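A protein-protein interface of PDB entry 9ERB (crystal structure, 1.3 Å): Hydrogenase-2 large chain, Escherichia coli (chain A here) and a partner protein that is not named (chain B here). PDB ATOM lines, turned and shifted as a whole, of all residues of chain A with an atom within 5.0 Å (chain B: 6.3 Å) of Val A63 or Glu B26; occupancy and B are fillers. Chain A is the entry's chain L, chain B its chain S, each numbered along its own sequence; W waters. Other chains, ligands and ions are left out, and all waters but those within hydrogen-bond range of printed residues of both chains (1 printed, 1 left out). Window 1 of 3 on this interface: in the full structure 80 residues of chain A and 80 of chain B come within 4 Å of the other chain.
The side-chain sulfur (SG) of Cys B21 sits close to the backbone NH (N) of Gly B23. OG of Ser B27 is in hydrogen-bond range of O of Cys B24 (2.8 Å). The side-chain carboxylate (OE1) of Glu B26 is in salt-bridge range of the guanidinium group (NH1) of Arg B30 (2.9 Å). The side-chain sulfur (SG) of Cys A546 lies close to the side-chain carboxylate (OE1) of Glu A14 (3.4 Å). The side-chain sulfur (SG) of Cys A61 sits close to the backbone NH (N) of Val A63 (3.4 Å). The backbone carbonyl oxygen (O) of Val A63 sits close to a ring nitrogen (NE2) of His A99 (3.3 Å).
Water W1 bridges the side-chain carboxylate (OE2) of Glu B26 (2.6 Å) and a ring nitrogen (NE2) of His A102 (3.1 Å).
Of the printed residues of chain B, Gly A62 touches Cys B21, Gly B23 and Glu B26. Val A63 touches just these residues of chain B: Cys B21 (3.9 Å), Thr B22 (3.6 Å) and Glu B26 (3.4 Å). Of the printed residues of chain B, Pro A213 touches Gly B23 (3.4 Å), Glu B26 (3.8 Å), Ser B27 (3.8 Å), Arg B30 (3.4 Å) and Pro B154 (3.4 Å). Printed residues of chain A within 4 Å of Thr B22: Glu A14 (2.5 Å) and Val A63 (3.6 Å). Glu B26 touches four residues of chain A. Of the printed residues of chain A, Ser B27 touches Pro A213. Of the printed residues of chain A, Arg B30 touches His A102 (3.6 Å) and Pro A213 (3.4 Å). The nearest residue of chain B that does not touch Val A63 is Gly B23 (4.7 Å).
O of Cys B21 lies within hydrogen-bond range of N of Gly A62 (2.8 Å). OE2 of Glu A14 lies within hydrogen-bond range of OG1 of Thr B22 (2.5 Å). The side-chain carboxylate (OE2) of Glu A14 lies close to the backbone carbonyl oxygen (O) of Cys B21.
Hydrophobic or aromatic side chains of chain B that line the printed part of chain A: Pro B154. Along chain B the printed residues that touch a printed residue of chain A span positions 21 to 154. Along chain A the printed residues that touch a printed residue of chain B span positions 14 to 213. Among the printed residues, 16 pairs touch across the chains.
Among the printed residues, pairs that only touch across the chains: Cys A61 with Cys B21 (3.8 Å), Gly A62 with Gly B23 (3.7 Å), Gly A62 with Glu B26 (3.6 Å), Val A63 with Cys B21 (3.9 Å), Val A63 with Thr B22 (3.6 Å), Val A63 with Glu B26 (3.4 Å), His A102 with Glu B26 (3.4 Å), His A102 with Arg B30 (3.6 Å), Pro A213 with Gly B23 (3.4 Å), Pro A213 with Glu B26 (3.8 Å), Pro A213 with Ser B27 (3.8 Å), Pro A213 with Arg B30 (3.4 Å) and Pro A213 with Pro B154 (3.4 Å).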
ATOM      1  N   GLU A  14     -10.540   3.236   1.854  1.00  0.00           N
ATOM      2  CA  GLU A  14     -10.334   2.530   0.606  1.00  0.00           C
ATOM      3  C   GLU A  14      -8.956   1.881   0.621  1.00  0.00           C
ATOM      4  O   GLU A  14      -7.938   2.547   0.898  1.00  0.00           O
ATOM      5  CB  GLU A  14     -10.462   3.478  -0.582  1.00  0.00           C
ATOM      6  CG  GLU A  14     -10.455   2.767  -1.934  1.00  0.00           C
ATOM      7  CD  GLU A  14      -9.164   2.033  -2.304  1.00  0.00           C
ATOM      8  OE1 GLU A  14      -8.072   2.529  -1.952  1.00  0.00           O
ATOM      9  OE2 GLU A  14      -9.236   0.955  -2.979  1.00  0.00           O
ATOM     10  N   CYS A  61      -8.806   4.348  -8.897  1.00  0.00           N
ATOM     11  CA  CYS A  61      -9.679   4.338  -7.735  1.00  0.00           C
ATOM     12  C   CYS A  61     -11.150   4.433  -8.116  1.00  0.00           C
ATOM     13  O   CYS A  61     -11.527   5.287  -8.919  1.00  0.00           O
ATOM     14  CB  CYS A  61      -9.328   5.491  -6.787  1.00  0.00           C
ATOM     15  SG  CYS A  61     -10.200   5.362  -5.195  1.00  0.00           S
ATOM     16  N   GLY A  62     -11.957   3.581  -7.495  1.00  0.00           N
ATOM     17  CA  GLY A  62     -13.397   3.601  -7.659  1.00  0.00           C
ATOM     18  C   GLY A  62     -14.154   4.310  -6.568  1.00  0.00           C
ATOM     19  O   GLY A  62     -15.367   4.561  -6.728  1.00  0.00           O
ATOM     20  N   VAL A  63     -13.491   4.616  -5.445  1.00  0.00           N
ATOM     21  CA  VAL A  63     -14.121   5.481  -4.450  1.00  0.00           C
ATOM     22  C   VAL A  63     -14.095   6.904  -4.966  1.00  0.00           C
ATOM     23  O   VAL A  63     -15.144   7.503  -5.223  1.00  0.00           O
ATOM     24  CB  VAL A  63     -13.451   5.350  -3.070  1.00  0.00           C
ATOM     25  CG1 VAL A  63     -14.036   6.374  -2.084  1.00  0.00           C
ATOM     26  CG2 VAL A  63     -13.624   3.931  -2.562  1.00  0.00           C
ATOM     27  N   CYS A  64     -12.892   7.418  -5.230  1.00  0.00           N
ATOM     28  CA  CYS A  64     -12.755   8.686  -5.927  1.00  0.00           C
ATOM     29  C   CYS A  64     -12.776   8.467  -7.433  1.00  0.00           C
ATOM     30  O   CYS A  64     -11.910   8.923  -8.195  1.00  0.00           O
ATOM     31  CB  CYS A  64     -11.529   9.447  -5.450  1.00  0.00           C
ATOM     32  SG  CYS A  64      -9.933   8.706  -5.811  1.00  0.00           S
ATOM     33  N   THR A  65     -13.812   7.752  -7.877  1.00  0.00           N
ATOM     34  CA  THR A  65     -14.089   7.693  -9.296  1.00  0.00           C
ATOM     35  C   THR A  65     -14.284   9.123  -9.815  1.00  0.00           C
ATOM     36  O   THR A  65     -14.482  10.058  -9.038  1.00  0.00           O
ATOM     37  CB  THR A  65     -15.239   6.740  -9.582  1.00  0.00           C
ATOM     38  OG1 THR A  65     -15.309   6.526 -11.003  1.00  0.00           O
ATOM     39  CG2 THR A  65     -16.557   7.261  -9.099  1.00  0.00           C
ATOM     40  N   HIS A  99     -20.062  14.065  -7.545  1.00  0.00           N
ATOM     41  CA  HIS A  99     -19.296  12.939  -7.053  1.00  0.00           C
ATOM     42  C   HIS A  99     -18.782  13.224  -5.649  1.00  0.00           C
ATOM     43  O   HIS A  99     -18.864  12.384  -4.736  1.00  0.00           O
ATOM     44  CB  HIS A  99     -18.069  12.652  -7.930  1.00  0.00           C
ATOM     45  CG  HIS A  99     -17.197  11.668  -7.241  1.00  0.00           C
ATOM     46  ND1 HIS A  99     -17.521  10.328  -7.185  1.00  0.00           N
ATOM     47  CD2 HIS A  99     -16.185  11.856  -6.368  1.00  0.00           C
ATOM     48  CE1 HIS A  99     -16.709   9.730  -6.336  1.00  0.00           C
ATOM     49  NE2 HIS A  99     -15.883  10.633  -5.832  1.00  0.00           N
ATOM     50  N   HIS A 102     -21.344  12.804  -2.851  1.00  0.00           N
ATOM     51  CA  HIS A 102     -21.465  11.397  -2.459  1.00  0.00           C
ATOM     52  C   HIS A 102     -20.262  10.963  -1.638  1.00  0.00           C
ATOM     53  O   HIS A 102     -20.413  10.288  -0.611  1.00  0.00           O
ATOM     54  CB  HIS A 102     -21.573  10.526  -3.730  1.00  0.00           C
ATOM     55  CG  HIS A 102     -20.834   9.216  -3.682  1.00  0.00           C
ATOM     56  ND1 HIS A 102     -21.335   8.038  -3.156  1.00  0.00           N
ATOM     57  CD2 HIS A 102     -19.604   8.916  -4.142  1.00  0.00           C
ATOM     58  CE1 HIS A 102     -20.436   7.077  -3.301  1.00  0.00           C
ATOM     59  NE2 HIS A 102     -19.373   7.588  -3.885  1.00  0.00           N
ATOM     60  N   ASP A 103     -19.064  11.331  -2.081  1.00  0.00           N
ATOM     61  CA  ASP A 103     -17.830  10.830  -1.472  1.00  0.00           C
ATOM     62  C   ASP A 103     -17.741  11.286  -0.012  1.00  0.00           C
ATOM     63  O   ASP A 103     -17.589  10.465   0.917  1.00  0.00           O
ATOM     64  CB  ASP A 103     -16.664  11.306  -2.371  1.00  0.00           C
ATOM     65  CG  ASP A 103     -15.385  10.517  -2.212  1.00  0.00           C
ATOM     66  OD1 ASP A 103     -15.132  10.044  -1.092  1.00  0.00           O
ATOM     67  OD2 ASP A 103     -14.606  10.429  -3.188  1.00  0.00           O
ATOM     68  N   PRO A 213     -20.060   3.711 -10.615  1.00  0.00           N
ATOM     69  CA  PRO A 213     -18.658   4.089 -10.775  1.00  0.00           C
ATOM     70  C   PRO A 213     -18.125   4.034 -12.200  1.00  0.00           C
ATOM     71  O   PRO A 213     -18.595   3.277 -13.041  1.00  0.00           O
ATOM     72  CB  PRO A 213     -17.881   3.082  -9.874  1.00  0.00           C
ATOM     73  CG  PRO A 213     -18.918   2.573  -8.903  1.00  0.00           C
ATOM     74  CD  PRO A 213     -20.185   2.520  -9.731  1.00  0.00           C
ATOM     75  N   ARG A 479      -9.991  14.210  -1.530  1.00  0.00           N
ATOM     76  CA  ARG A 479      -8.924  14.028  -0.561  1.00  0.00           C
ATOM     77  C   ARG A 479      -7.774  15.018  -0.733  1.00  0.00           C
ATOM     78  O   ARG A 479      -6.828  14.982   0.057  1.00  0.00           O
ATOM     79  CB  ARG A 479      -8.473  12.584  -0.596  1.00  0.00           C
ATOM     80  CG  ARG A 479      -9.542  11.664  -0.027  1.00  0.00           C
ATOM     81  CD  ARG A 479      -9.377  10.235  -0.483  1.00  0.00           C
ATOM     82  NE  ARG A 479     -10.521   9.389  -0.108  1.00  0.00           N
ATOM     83  CZ  ARG A 479     -11.715   9.436  -0.687  1.00  0.00           C
ATOM     84  NH1 ARG A 479     -11.892  10.021  -1.852  1.00  0.00           N
ATOM     85  NH2 ARG A 479     -12.742   8.870  -0.097  1.00  0.00           N
ATOM     86  N   CYS A 546      -7.141   6.758   1.005  1.00  0.00           N
ATOM     87  CA  CYS A 546      -7.446   5.948  -0.177  1.00  0.00           C
ATOM     88  C   CYS A 546      -6.117   5.380  -0.650  1.00  0.00           C
ATOM     89  O   CYS A 546      -5.282   6.106  -1.211  1.00  0.00           O
ATOM     90  CB  CYS A 546      -8.090   6.809  -1.229  1.00  0.00           C
ATOM     91  SG  CYS A 546      -8.620   5.828  -2.639  1.00  0.00           S
ATOM     92  N   CYS B  21      -9.806  -1.572  -6.937  1.00  0.00           N
ATOM     93  CA  CYS B  21      -9.905  -0.130  -6.863  1.00  0.00           C
ATOM     94  C   CYS B  21     -11.075   0.309  -5.991  1.00  0.00           C
ATOM     95  O   CYS B  21     -11.231   1.505  -5.753  1.00  0.00           O
ATOM     96  CB  CYS B  21     -10.036   0.499  -8.258  1.00  0.00           C
ATOM     97  SG  CYS B  21     -11.729   0.450  -8.935  1.00  0.00           S
ATOM     98  N   THR B  22     -11.891  -0.631  -5.514  1.00  0.00           N
ATOM     99  CA  THR B  22     -13.087  -0.459  -4.684  1.00  0.00           C
ATOM    100  C   THR B  22     -14.319  -0.056  -5.492  1.00  0.00           C
ATOM    101  O   THR B  22     -15.430  -0.027  -4.949  1.00  0.00           O
ATOM    102  CB  THR B  22     -12.823   0.438  -3.468  1.00  0.00           C
ATOM    103  OG1 THR B  22     -11.582   0.000  -2.874  1.00  0.00           O
ATOM    104  CG2 THR B  22     -13.893   0.327  -2.423  1.00  0.00           C
ATOM    105  N   GLY B  23     -14.187   0.136  -6.803  1.00  0.00           N
ATOM    106  CA  GLY B  23     -15.339   0.437  -7.629  1.00  0.00           C
ATOM    107  C   GLY B  23     -16.392  -0.646  -7.610  1.00  0.00           C
ATOM    108  O   GLY B  23     -17.588  -0.368  -7.763  1.00  0.00           O
ATOM    109  N   CYS B  24     -16.001  -1.903  -7.441  1.00  0.00           N
ATOM    110  CA  CYS B  24     -16.966  -2.998  -7.412  1.00  0.00           C
ATOM    111  C   CYS B  24     -17.784  -2.995  -6.131  1.00  0.00           C
ATOM    112  O   CYS B  24     -18.995  -3.189  -6.163  1.00  0.00           O
ATOM    113  CB  CYS B  24     -16.254  -4.345  -7.647  1.00  0.00           C
ATOM    114  SG  CYS B  24     -15.657  -4.619  -9.356  1.00  0.00           S
ATOM    115  N   THR B  25     -17.158  -2.729  -4.981  1.00  0.00           N
ATOM    116  CA  THR B  25     -17.944  -2.465  -3.780  1.00  0.00           C
ATOM    117  C   THR B  25     -18.819  -1.230  -3.964  1.00  0.00           C
ATOM    118  O   THR B  25     -19.993  -1.215  -3.567  1.00  0.00           O
ATOM    119  CB  THR B  25     -17.012  -2.295  -2.578  1.00  0.00           C
ATOM    120  OG1 THR B  25     -16.444  -3.576  -2.256  1.00  0.00           O
ATOM    121  CG2 THR B  25     -17.757  -1.737  -1.411  1.00  0.00           C
ATOM    122  N   GLU B  26     -18.260  -0.164  -4.535  1.00  0.00           N
ATOM    123  CA  GLU B  26     -19.012   1.074  -4.678  1.00  0.00           C
ATOM    124  C   GLU B  26     -20.242   0.894  -5.554  1.00  0.00           C
ATOM    125  O   GLU B  26     -21.228   1.612  -5.378  1.00  0.00           O
ATOM    126  CB  GLU B  26     -18.105   2.155  -5.257  1.00  0.00           C
ATOM    127  CG  GLU B  26     -17.169   2.748  -4.247  1.00  0.00           C
ATOM    128  CD  GLU B  26     -17.797   3.765  -3.337  1.00  0.00           C
ATOM    129  OE1 GLU B  26     -19.010   4.041  -3.437  1.00  0.00           O
ATOM    130  OE2 GLU B  26     -17.012   4.284  -2.450  1.00  0.00           O
ATOM    131  N   SER B  27     -20.223  -0.066  -6.486  1.00  0.00           N
ATOM    132  CA  SER B  27     -21.418  -0.302  -7.286  1.00  0.00           C
ATOM    133  C   SER B  27     -22.628  -0.574  -6.390  1.00  0.00           C
ATOM    134  O   SER B  27     -23.759  -0.151  -6.703  1.00  0.00           O
ATOM    135  CB  SER B  27     -21.242  -1.437  -8.300  1.00  0.00           C
ATOM    136  OG  SER B  27     -21.243  -2.718  -7.725  1.00  0.00           O
ATOM    137  N   LEU B  28     -22.403  -1.245  -5.261  1.00  0.00           N
ATOM    138  CA  LEU B  28     -23.489  -1.578  -4.352  1.00  0.00           C
ATOM    139  C   LEU B  28     -24.170  -0.337  -3.809  1.00  0.00           C
ATOM    140  O   LEU B  28     -25.355  -0.390  -3.470  1.00  0.00           O
ATOM    141  CB  LEU B  28     -22.959  -2.383  -3.172  1.00  0.00           C
ATOM    142  CG  LEU B  28     -22.302  -3.704  -3.537  1.00  0.00           C
ATOM    143  CD1 LEU B  28     -21.892  -4.393  -2.223  1.00  0.00           C
ATOM    144  CD2 LEU B  28     -23.214  -4.570  -4.366  1.00  0.00           C
ATOM    145  N   LEU B  29     -23.438   0.767  -3.688  1.00  0.00           N
ATOM    146  CA  LEU B  29     -23.999   2.008  -3.176  1.00  0.00           C
ATOM    147  C   LEU B  29     -24.916   2.693  -4.167  1.00  0.00           C
ATOM    148  O   LEU B  29     -25.649   3.595  -3.756  1.00  0.00           O
ATOM    149  CB  LEU B  29     -22.895   2.973  -2.682  1.00  0.00           C
ATOM    150  CG  LEU B  29     -22.486   2.735  -1.215  1.00  0.00           C
ATOM    151  CD1 LEU B  29     -21.878   1.380  -0.992  1.00  0.00           C
ATOM    152  CD2 LEU B  29     -21.539   3.837  -0.750  1.00  0.00           C
ATOM    153  N   ARG B  30     -24.954   2.248  -5.417  1.00  0.00           N
ATOM    154  CA  ARG B  30     -25.928   2.749  -6.385  1.00  0.00           C
ATOM    155  C   ARG B  30     -27.140   1.825  -6.505  1.00  0.00           C
ATOM    156  O   ARG B  30     -28.146   2.195  -7.125  1.00  0.00           O
ATOM    157  CB  ARG B  30     -25.288   2.875  -7.777  1.00  0.00           C
ATOM    158  CG  ARG B  30     -24.280   4.005  -7.950  1.00  0.00           C
ATOM    159  CD  ARG B  30     -22.982   3.767  -7.184  1.00  0.00           C
ATOM    160  NE  ARG B  30     -21.924   4.643  -7.672  1.00  0.00           N
ATOM    161  CZ  ARG B  30     -20.851   4.968  -6.973  1.00  0.00           C
ATOM    162  NH1 ARG B  30     -20.667   4.518  -5.758  1.00  0.00           N
ATOM    163  NH2 ARG B  30     -19.951   5.783  -7.496  1.00  0.00           N
ATOM    164  N   ALA B  31     -27.055   0.612  -5.982  1.00  0.00           N
ATOM    165  CA  ALA B  31     -28.115  -0.365  -6.181  1.00  0.00           C
ATOM    166  C   ALA B  31     -29.405   0.063  -5.505  1.00  0.00           C
ATOM    167  O   ALA B  31     -29.410   0.791  -4.521  1.00  0.00           O
ATOM    168  CB  ALA B  31     -27.689  -1.700  -5.588  1.00  0.00           C
ATOM    169  N   VAL B  51     -14.385  -2.523   3.827  1.00  0.00           N
ATOM    170  CA  VAL B  51     -14.737  -1.128   3.596  1.00  0.00           C
ATOM    171  C   VAL B  51     -15.737  -0.650   4.641  1.00  0.00           C
ATOM    172  O   VAL B  51     -15.766   0.541   4.972  1.00  0.00           O
ATOM    173  CB  VAL B  51     -15.286  -0.942   2.167  1.00  0.00           C
ATOM    174  CG1 VAL B  51     -15.842   0.467   1.926  1.00  0.00           C
ATOM    175  CG2 VAL B  51     -14.205  -1.263   1.133  1.00  0.00           C
ATOM    176  N   PRO B 154     -17.069  -1.132 -13.039  1.00  0.00           N
ATOM    177  CA  PRO B 154     -17.621  -2.347 -12.448  1.00  0.00           C
ATOM    178  C   PRO B 154     -18.907  -2.732 -13.146  1.00  0.00           C
ATOM    179  O   PRO B 154     -19.545  -1.944 -13.857  1.00  0.00           O
ATOM    180  CB  PRO B 154     -17.950  -1.912 -11.028  1.00  0.00           C
ATOM    181  CG  PRO B 154     -18.379  -0.440 -11.211  1.00  0.00           C
ATOM    182  CD  PRO B 154     -17.522   0.079 -12.349  1.00  0.00           C
HETATM  183  O   HOH W   1     -17.923   6.515  -1.421  1.00  0.00           O
